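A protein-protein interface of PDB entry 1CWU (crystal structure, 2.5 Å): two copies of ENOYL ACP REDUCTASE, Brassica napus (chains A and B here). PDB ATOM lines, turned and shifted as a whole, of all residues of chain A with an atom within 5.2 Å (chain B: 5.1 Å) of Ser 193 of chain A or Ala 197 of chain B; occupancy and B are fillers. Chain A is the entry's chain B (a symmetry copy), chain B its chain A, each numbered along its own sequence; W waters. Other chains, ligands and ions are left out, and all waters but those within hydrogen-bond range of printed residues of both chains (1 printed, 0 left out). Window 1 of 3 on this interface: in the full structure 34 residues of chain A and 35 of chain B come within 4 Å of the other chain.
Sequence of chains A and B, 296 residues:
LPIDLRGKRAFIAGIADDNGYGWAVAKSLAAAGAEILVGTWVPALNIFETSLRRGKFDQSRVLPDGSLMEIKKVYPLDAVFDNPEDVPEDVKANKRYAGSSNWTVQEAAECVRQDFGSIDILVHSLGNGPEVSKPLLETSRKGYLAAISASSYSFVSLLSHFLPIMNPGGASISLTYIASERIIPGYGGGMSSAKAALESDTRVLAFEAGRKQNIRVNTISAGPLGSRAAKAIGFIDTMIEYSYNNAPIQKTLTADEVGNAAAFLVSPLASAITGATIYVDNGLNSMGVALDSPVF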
ATOM      1  N   LEU A 136      -4.756  -6.312 -14.883  1.00  0.00           N
ATOM      2  CA  LEU A 136      -4.732  -6.249 -16.341  1.00  0.00           C
ATOM      3  C   LEU A 136      -5.212  -4.873 -16.810  1.00  0.00           C
ATOM      4  O   LEU A 136      -4.692  -4.307 -17.772  1.00  0.00           O
ATOM      5  CB  LEU A 136      -5.592  -7.349 -16.963  1.00  0.00           C
ATOM      6  CG  LEU A 136      -4.888  -8.669 -17.278  1.00  0.00           C
ATOM      7  CD1 LEU A 136      -5.836  -9.594 -17.999  1.00  0.00           C
ATOM      8  CD2 LEU A 136      -3.655  -8.465 -18.123  1.00  0.00           C
ATOM      9  N   TYR A 144       2.962  -6.058 -20.278  1.00  0.00           N
ATOM     10  CA  TYR A 144       2.297  -7.274 -20.696  1.00  0.00           C
ATOM     11  C   TYR A 144       3.224  -8.056 -21.556  1.00  0.00           C
ATOM     12  O   TYR A 144       3.455  -9.233 -21.306  1.00  0.00           O
ATOM     13  CB  TYR A 144       1.099  -6.898 -21.542  1.00  0.00           C
ATOM     14  CG  TYR A 144       0.096  -8.010 -21.861  1.00  0.00           C
ATOM     15  CD1 TYR A 144       0.133  -8.683 -23.072  1.00  0.00           C
ATOM     16  CD2 TYR A 144      -0.997  -8.226 -21.044  1.00  0.00           C
ATOM     17  CE1 TYR A 144      -0.836  -9.609 -23.416  1.00  0.00           C
ATOM     18  CE2 TYR A 144      -1.990  -9.143 -21.389  1.00  0.00           C
ATOM     19  CZ  TYR A 144      -1.908  -9.827 -22.571  1.00  0.00           C
ATOM     20  OH  TYR A 144      -2.904 -10.746 -22.884  1.00  0.00           O
ATOM     21  N   ILE A 148       5.198 -11.571 -21.109  1.00  0.00           N
ATOM     22  CA  ILE A 148       4.986 -12.700 -22.003  1.00  0.00           C
ATOM     23  C   ILE A 148       6.297 -13.117 -22.637  1.00  0.00           C
ATOM     24  O   ILE A 148       6.496 -14.286 -22.990  1.00  0.00           O
ATOM     25  CB  ILE A 148       3.959 -12.331 -23.108  1.00  0.00           C
ATOM     26  CG1 ILE A 148       2.643 -11.869 -22.482  1.00  0.00           C
ATOM     27  CG2 ILE A 148       3.605 -13.552 -23.943  1.00  0.00           C
ATOM     28  CD1 ILE A 148       1.577 -12.905 -22.588  1.00  0.00           C
ATOM     29  N   SER A 152       6.853 -16.536 -21.272  1.00  0.00           N
ATOM     30  CA  SER A 152       6.359 -17.537 -22.238  1.00  0.00           C
ATOM     31  C   SER A 152       7.341 -17.787 -23.377  1.00  0.00           C
ATOM     32  O   SER A 152       7.855 -18.896 -23.522  1.00  0.00           O
ATOM     33  CB  SER A 152       4.972 -17.179 -22.821  1.00  0.00           C
ATOM     34  OG  SER A 152       4.005 -16.983 -21.810  1.00  0.00           O
ATOM     35  N   GLY A 190      -0.075  -9.229 -16.581  1.00  0.00           N
ATOM     36  CA  GLY A 190      -0.186 -10.140 -17.731  1.00  0.00           C
ATOM     37  C   GLY A 190       0.582 -11.460 -17.498  1.00  0.00           C
ATOM     38  O   GLY A 190       0.754 -12.270 -18.420  1.00  0.00           O
ATOM     39  N   MET A 191       1.024 -11.680 -16.255  1.00  0.00           N
ATOM     40  CA  MET A 191       1.730 -12.909 -15.900  1.00  0.00           C
ATOM     41  C   MET A 191       0.802 -14.057 -16.134  1.00  0.00           C
ATOM     42  O   MET A 191       1.180 -15.049 -16.745  1.00  0.00           O
ATOM     43  CB  MET A 191       2.174 -12.899 -14.450  1.00  0.00           C
ATOM     44  CG  MET A 191       3.491 -12.186 -14.227  1.00  0.00           C
ATOM     45  SD  MET A 191       4.751 -12.806 -15.331  1.00  0.00           S
ATOM     46  CE  MET A 191       5.063 -14.430 -14.596  1.00  0.00           C
ATOM     47  N   SER A 192      -0.450 -13.877 -15.720  1.00  0.00           N
ATOM     48  CA  SER A 192      -1.493 -14.881 -15.926  1.00  0.00           C
ATOM     49  C   SER A 192      -1.592 -15.188 -17.405  1.00  0.00           C
ATOM     50  O   SER A 192      -1.615 -16.349 -17.812  1.00  0.00           O
ATOM     51  CB  SER A 192      -2.826 -14.356 -15.400  1.00  0.00           C
ATOM     52  OG  SER A 192      -3.300 -13.294 -16.200  1.00  0.00           O
ATOM     53  N   SER A 193      -1.549 -14.143 -18.225  1.00  0.00           N
ATOM     54  CA  SER A 193      -1.618 -14.303 -19.676  1.00  0.00           C
ATOM     55  C   SER A 193      -0.416 -15.069 -20.149  1.00  0.00           C
ATOM     56  O   SER A 193      -0.482 -15.881 -21.099  1.00  0.00           O
ATOM     57  CB  SER A 193      -1.617 -12.937 -20.316  1.00  0.00           C
ATOM     58  OG  SER A 193      -2.290 -12.028 -19.471  1.00  0.00           O
ATOM     59  N   ALA A 194       0.701 -14.794 -19.489  1.00  0.00           N
ATOM     60  CA  ALA A 194       1.983 -15.435 -19.812  1.00  0.00           C
ATOM     61  C   ALA A 194       1.941 -16.933 -19.556  1.00  0.00           C
ATOM     62  O   ALA A 194       2.406 -17.709 -20.364  1.00  0.00           O
ATOM     63  CB  ALA A 194       3.068 -14.819 -18.996  1.00  0.00           C
ATOM     64  N   LYS A 195       1.377 -17.329 -18.412  1.00  0.00           N
ATOM     65  CA  LYS A 195       1.235 -18.742 -18.071  1.00  0.00           C
ATOM     66  C   LYS A 195       0.318 -19.421 -19.080  1.00  0.00           C
ATOM     67  O   LYS A 195       0.639 -20.466 -19.633  1.00  0.00           O
ATOM     68  CB  LYS A 195       0.691 -18.907 -16.654  1.00  0.00           C
ATOM     69  CG  LYS A 195       1.625 -18.451 -15.567  1.00  0.00           C
ATOM     70  CD  LYS A 195       3.048 -18.987 -15.809  1.00  0.00           C
ATOM     71  CE  LYS A 195       3.965 -18.718 -14.609  1.00  0.00           C
ATOM     72  NZ  LYS A 195       5.418 -19.012 -14.903  1.00  0.00           N
ATOM     73  N   ALA A 196      -0.811 -18.793 -19.361  1.00  0.00           N
ATOM     74  CA  ALA A 196      -1.723 -19.366 -20.331  1.00  0.00           C
ATOM     75  C   ALA A 196      -0.959 -19.661 -21.604  1.00  0.00           C
ATOM     76  O   ALA A 196      -1.068 -20.744 -22.181  1.00  0.00           O
ATOM     77  CB  ALA A 196      -2.859 -18.445 -20.593  1.00  0.00           C
ATOM     78  N   ALA A 197      -0.143 -18.713 -22.030  1.00  0.00           N
ATOM     79  CA  ALA A 197       0.632 -18.920 -23.257  1.00  0.00           C
ATOM     80  C   ALA A 197       1.668 -20.047 -23.085  1.00  0.00           C
ATOM     81  O   ALA A 197       1.838 -20.889 -23.965  1.00  0.00           O
ATOM     82  CB  ALA A 197       1.291 -17.616 -23.693  1.00  0.00           C
ATOM     83  N   LEU A 198       2.334 -20.067 -21.933  1.00  0.00           N
ATOM     84  CA  LEU A 198       3.339 -21.080 -21.655  1.00  0.00           C
ATOM     85  C   LEU A 198       2.648 -22.439 -21.661  1.00  0.00           C
ATOM     86  O   LEU A 198       3.185 -23.426 -22.175  1.00  0.00           O
ATOM     87  CB  LEU A 198       4.024 -20.814 -20.299  1.00  0.00           C
ATOM     88  CG  LEU A 198       5.035 -21.836 -19.747  1.00  0.00           C
ATOM     89  CD1 LEU A 198       6.219 -22.032 -20.655  1.00  0.00           C
ATOM     90  CD2 LEU A 198       5.481 -21.471 -18.376  1.00  0.00           C
ATOM     91  N   SER B 152      -4.082 -10.126 -28.801  1.00  0.00           N
ATOM     92  CA  SER B 152      -4.372 -10.353 -27.422  1.00  0.00           C
ATOM     93  C   SER B 152      -4.383  -9.083 -26.565  1.00  0.00           C
ATOM     94  O   SER B 152      -5.413  -8.709 -26.021  1.00  0.00           O
ATOM     95  CB  SER B 152      -3.419 -11.433 -26.896  1.00  0.00           C
ATOM     96  OG  SER B 152      -3.370 -11.412 -25.485  1.00  0.00           O
ATOM     97  N   SER B 193      -0.714 -19.197 -29.016  1.00  0.00           N
ATOM     98  CA  SER B 193      -0.385 -18.632 -27.729  1.00  0.00           C
ATOM     99  C   SER B 193      -1.283 -17.442 -27.434  1.00  0.00           C
ATOM    100  O   SER B 193      -1.679 -17.229 -26.298  1.00  0.00           O
ATOM    101  CB  SER B 193       1.065 -18.189 -27.734  1.00  0.00           C
ATOM    102  OG  SER B 193       1.825 -19.039 -28.555  1.00  0.00           O
ATOM    103  N   ALA B 194      -1.609 -16.673 -28.468  1.00  0.00           N
ATOM    104  CA  ALA B 194      -2.440 -15.463 -28.322  1.00  0.00           C
ATOM    105  C   ALA B 194      -3.869 -15.692 -27.845  1.00  0.00           C
ATOM    106  O   ALA B 194      -4.376 -14.942 -26.993  1.00  0.00           O
ATOM    107  CB  ALA B 194      -2.435 -14.655 -29.621  1.00  0.00           C
ATOM    108  N   LYS B 195      -4.541 -16.697 -28.406  1.00  0.00           N
ATOM    109  CA  LYS B 195      -5.929 -16.989 -27.991  1.00  0.00           C
ATOM    110  C   LYS B 195      -5.923 -17.454 -26.558  1.00  0.00           C
ATOM    111  O   LYS B 195      -6.780 -17.090 -25.760  1.00  0.00           O
ATOM    112  CB  LYS B 195      -6.547 -18.079 -28.855  1.00  0.00           C
ATOM    113  CG  LYS B 195      -6.644 -17.727 -30.315  1.00  0.00           C
ATOM    114  CD  LYS B 195      -7.251 -16.342 -30.527  1.00  0.00           C
ATOM    115  CE  LYS B 195      -7.712 -16.193 -31.981  1.00  0.00           C
ATOM    116  NZ  LYS B 195      -8.238 -14.827 -32.275  1.00  0.00           N
ATOM    117  N   ALA B 196      -4.923 -18.246 -26.230  1.00  0.00           N
ATOM    118  CA  ALA B 196      -4.800 -18.739 -24.876  1.00  0.00           C
ATOM    119  C   ALA B 196      -4.880 -17.570 -23.925  1.00  0.00           C
ATOM    120  O   ALA B 196      -5.675 -17.575 -22.973  1.00  0.00           O
ATOM    121  CB  ALA B 196      -3.478 -19.477 -24.693  1.00  0.00           C
ATOM    122  N   ALA B 197      -4.062 -16.553 -24.187  1.00  0.00           N
ATOM    123  CA  ALA B 197      -4.028 -15.361 -23.319  1.00  0.00           C
ATOM    124  C   ALA B 197      -5.296 -14.525 -23.405  1.00  0.00           C
ATOM    125  O   ALA B 197      -5.732 -13.929 -22.411  1.00  0.00           O
ATOM    126  CB  ALA B 197      -2.834 -14.525 -23.641  1.00  0.00           C
ATOM    127  N   LEU B 198      -5.880 -14.465 -24.604  1.00  0.00           N
ATOM    128  CA  LEU B 198      -7.109 -13.714 -24.821  1.00  0.00           C
ATOM    129  C   LEU B 198      -8.181 -14.345 -23.907  1.00  0.00           C
ATOM    130  O   LEU B 198      -8.857 -13.664 -23.109  1.00  0.00           O
ATOM    131  CB  LEU B 198      -7.494 -13.846 -26.296  1.00  0.00           C
ATOM    132  CG  LEU B 198      -8.805 -13.225 -26.769  1.00  0.00           C
ATOM    133  CD1 LEU B 198      -8.760 -11.680 -26.748  1.00  0.00           C
ATOM    134  CD2 LEU B 198      -9.144 -13.747 -28.140  1.00  0.00           C
ATOM    135  N   GLU B 199      -8.259 -15.677 -23.971  1.00  0.00           N
ATOM    136  CA  GLU B 199      -9.197 -16.442 -23.154  1.00  0.00           C
ATOM    137  C   GLU B 199      -8.854 -16.270 -21.663  1.00  0.00           C
ATOM    138  O   GLU B 199      -9.704 -15.970 -20.814  1.00  0.00           O
ATOM    139  CB  GLU B 199      -9.131 -17.912 -23.550  1.00  0.00           C
ATOM    140  CG  GLU B 199      -9.565 -18.234 -24.994  1.00  0.00           C
ATOM    141  CD  GLU B 199      -9.498 -19.736 -25.274  1.00  0.00           C
ATOM    142  OE1 GLU B 199      -9.165 -20.464 -24.314  1.00  0.00           O
ATOM    143  OE2 GLU B 199      -9.767 -20.186 -26.431  1.00  0.00           O
ATOM    144  N   SER B 200      -7.593 -16.410 -21.330  1.00  0.00           N
ATOM    145  CA  SER B 200      -7.258 -16.201 -19.950  1.00  0.00           C
ATOM    146  C   SER B 200      -7.661 -14.812 -19.516  1.00  0.00           C
ATOM    147  O   SER B 200      -8.257 -14.650 -18.466  1.00  0.00           O
ATOM    148  CB  SER B 200      -5.776 -16.430 -19.691  1.00  0.00           C
ATOM    149  OG  SER B 200      -5.463 -16.097 -18.349  1.00  0.00           O
ATOM    150  N   ASP B 201      -7.359 -13.803 -20.331  1.00  0.00           N
ATOM    151  CA  ASP B 201      -7.683 -12.410 -19.961  1.00  0.00           C
ATOM    152  C   ASP B 201      -9.166 -12.192 -19.747  1.00  0.00           C
ATOM    153  O   ASP B 201      -9.565 -11.411 -18.884  1.00  0.00           O
ATOM    154  CB  ASP B 201      -7.120 -11.400 -20.966  1.00  0.00           C
ATOM    155  CG  ASP B 201      -5.588 -11.434 -21.050  1.00  0.00           C
ATOM    156  OD1 ASP B 201      -4.954 -12.109 -20.196  1.00  0.00           O
ATOM    157  OD2 ASP B 201      -5.026 -10.865 -22.020  1.00  0.00           O
ATOM    158  N   THR B 202      -9.978 -12.927 -20.512  1.00  0.00           N
ATOM    159  CA  THR B 202     -11.442 -12.873 -20.393  1.00  0.00           C
ATOM    160  C   THR B 202     -11.863 -13.176 -18.963  1.00  0.00           C
ATOM    161  O   THR B 202     -12.665 -12.458 -18.376  1.00  0.00           O
ATOM    162  CB  THR B 202     -12.099 -13.904 -21.302  1.00  0.00           C
ATOM    163  OG1 THR B 202     -11.742 -13.645 -22.666  1.00  0.00           O
ATOM    164  CG2 THR B 202     -13.604 -13.886 -21.147  1.00  0.00           C
HETATM  165  O   HOH W   1      -5.017 -13.552 -18.068  1.00  0.00           O
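Of the 13 printed residues of chain A, 6 touch a printed residue of chain B. Hydrophobic or aromatic side chains of chain A within 4 Å of the printed part of chain B: Leu 136, Tyr 144, Ala 196 and Ala 197. Printed residues of chain B that touch a printed residue of chain A: Ser 152, Ser 193, Ala 196, Ala 197, Ser 200 and Asp 201. Along chain B the printed residues that touch a printed residue of chain A span positions 152 to 201.
Leu 136 of chain A touches Asp 201 of chain B (CD1 to OD1, 3.5 Å). Tyr 144 of chain A touches Ala 197 of chain B. Ser 200 of chain B touches Ser 192 of chain A. Ser 193 of chain A touches Ala 197 of chain B (O to CB, 3.7 Å). Ala 196 of chain B touches Ala 196 of chain A. Ala 196 of chain A touches Ser 200 of chain B. Ala 197 of chain A touches Ser 193 of chain B.
Water W1 lies within hydrogen-bond range of the side-chain hydroxyl (OG) of Ser 192 of chain A, the side-chain carboxylate (OD1) of Asp 201 of chain B, the side-chain hydroxyl (OG) of Ser 200 of chain B and the side-chain hydroxyl (OG) of Ser 193 of chain A.
Of chain B, only Ala 197 (3.7 Å) and Asp 201 (2.8 Å) come within 4 Å of Ser 193 of chain A. Of chain A, only Tyr 144 and Ser 193 come within 4 Å of Ala 197 of chain B. Of the printed residues of chain A, Asp 201 of chain B touches Leu 136, Tyr 144 and Ser 193. Printed residues of chain B within 4 Å of Leu 136 of chain A: Asp 201. Of the printed residues of chain A, Ala 196 of chain B touches Ala 196. Printed residues of chain A within 4 Å of Ser 200 of chain B: Ser 192 and Ala 196. Lys 195 of chain A touches none of the printed residues of chain B. Lys 195 of chain B touches none of the printed residues of chain A. The nearest printed residue of chain B that does not touch Ala 197 of chain A is Ala 196 of chain B (4.3 Å).
The side-chain hydroxyl (OG) of Ser 152 of chain B sits at hydrogen-bond distance from the side-chain hydroxyl (OH) of Tyr 144 of chain A (2.7 Å). OG of Ser 193 of chain A is in hydrogen-bond range of OD1 of Asp 201 of chain B (2.8 Å). The side-chain hydroxyl (OH) of Tyr 144 of chain A lies close to the side-chain carboxylate (OD2) of Asp 201 of chain B.
The backbone carbonyl oxygen of Gly 190 of chain A lies close to the side-chain hydroxyl of Ser 193 of chain A (3.2 Å).
Ser 193 of chain A touches Ala 197 of chain B, and with the chains exchanged Ala 197 of chain A touches Ser 193 of chain B. Ala 196 of chain A touches its own counterpart, Ala 196 of chain B. Positions printed for both chains: 152, 193, 194, 195, 196, 197 and 198. Of the 10 pairs that touch across the chains among the printed residues, 3 have their exchanged pair printed and touching as well.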
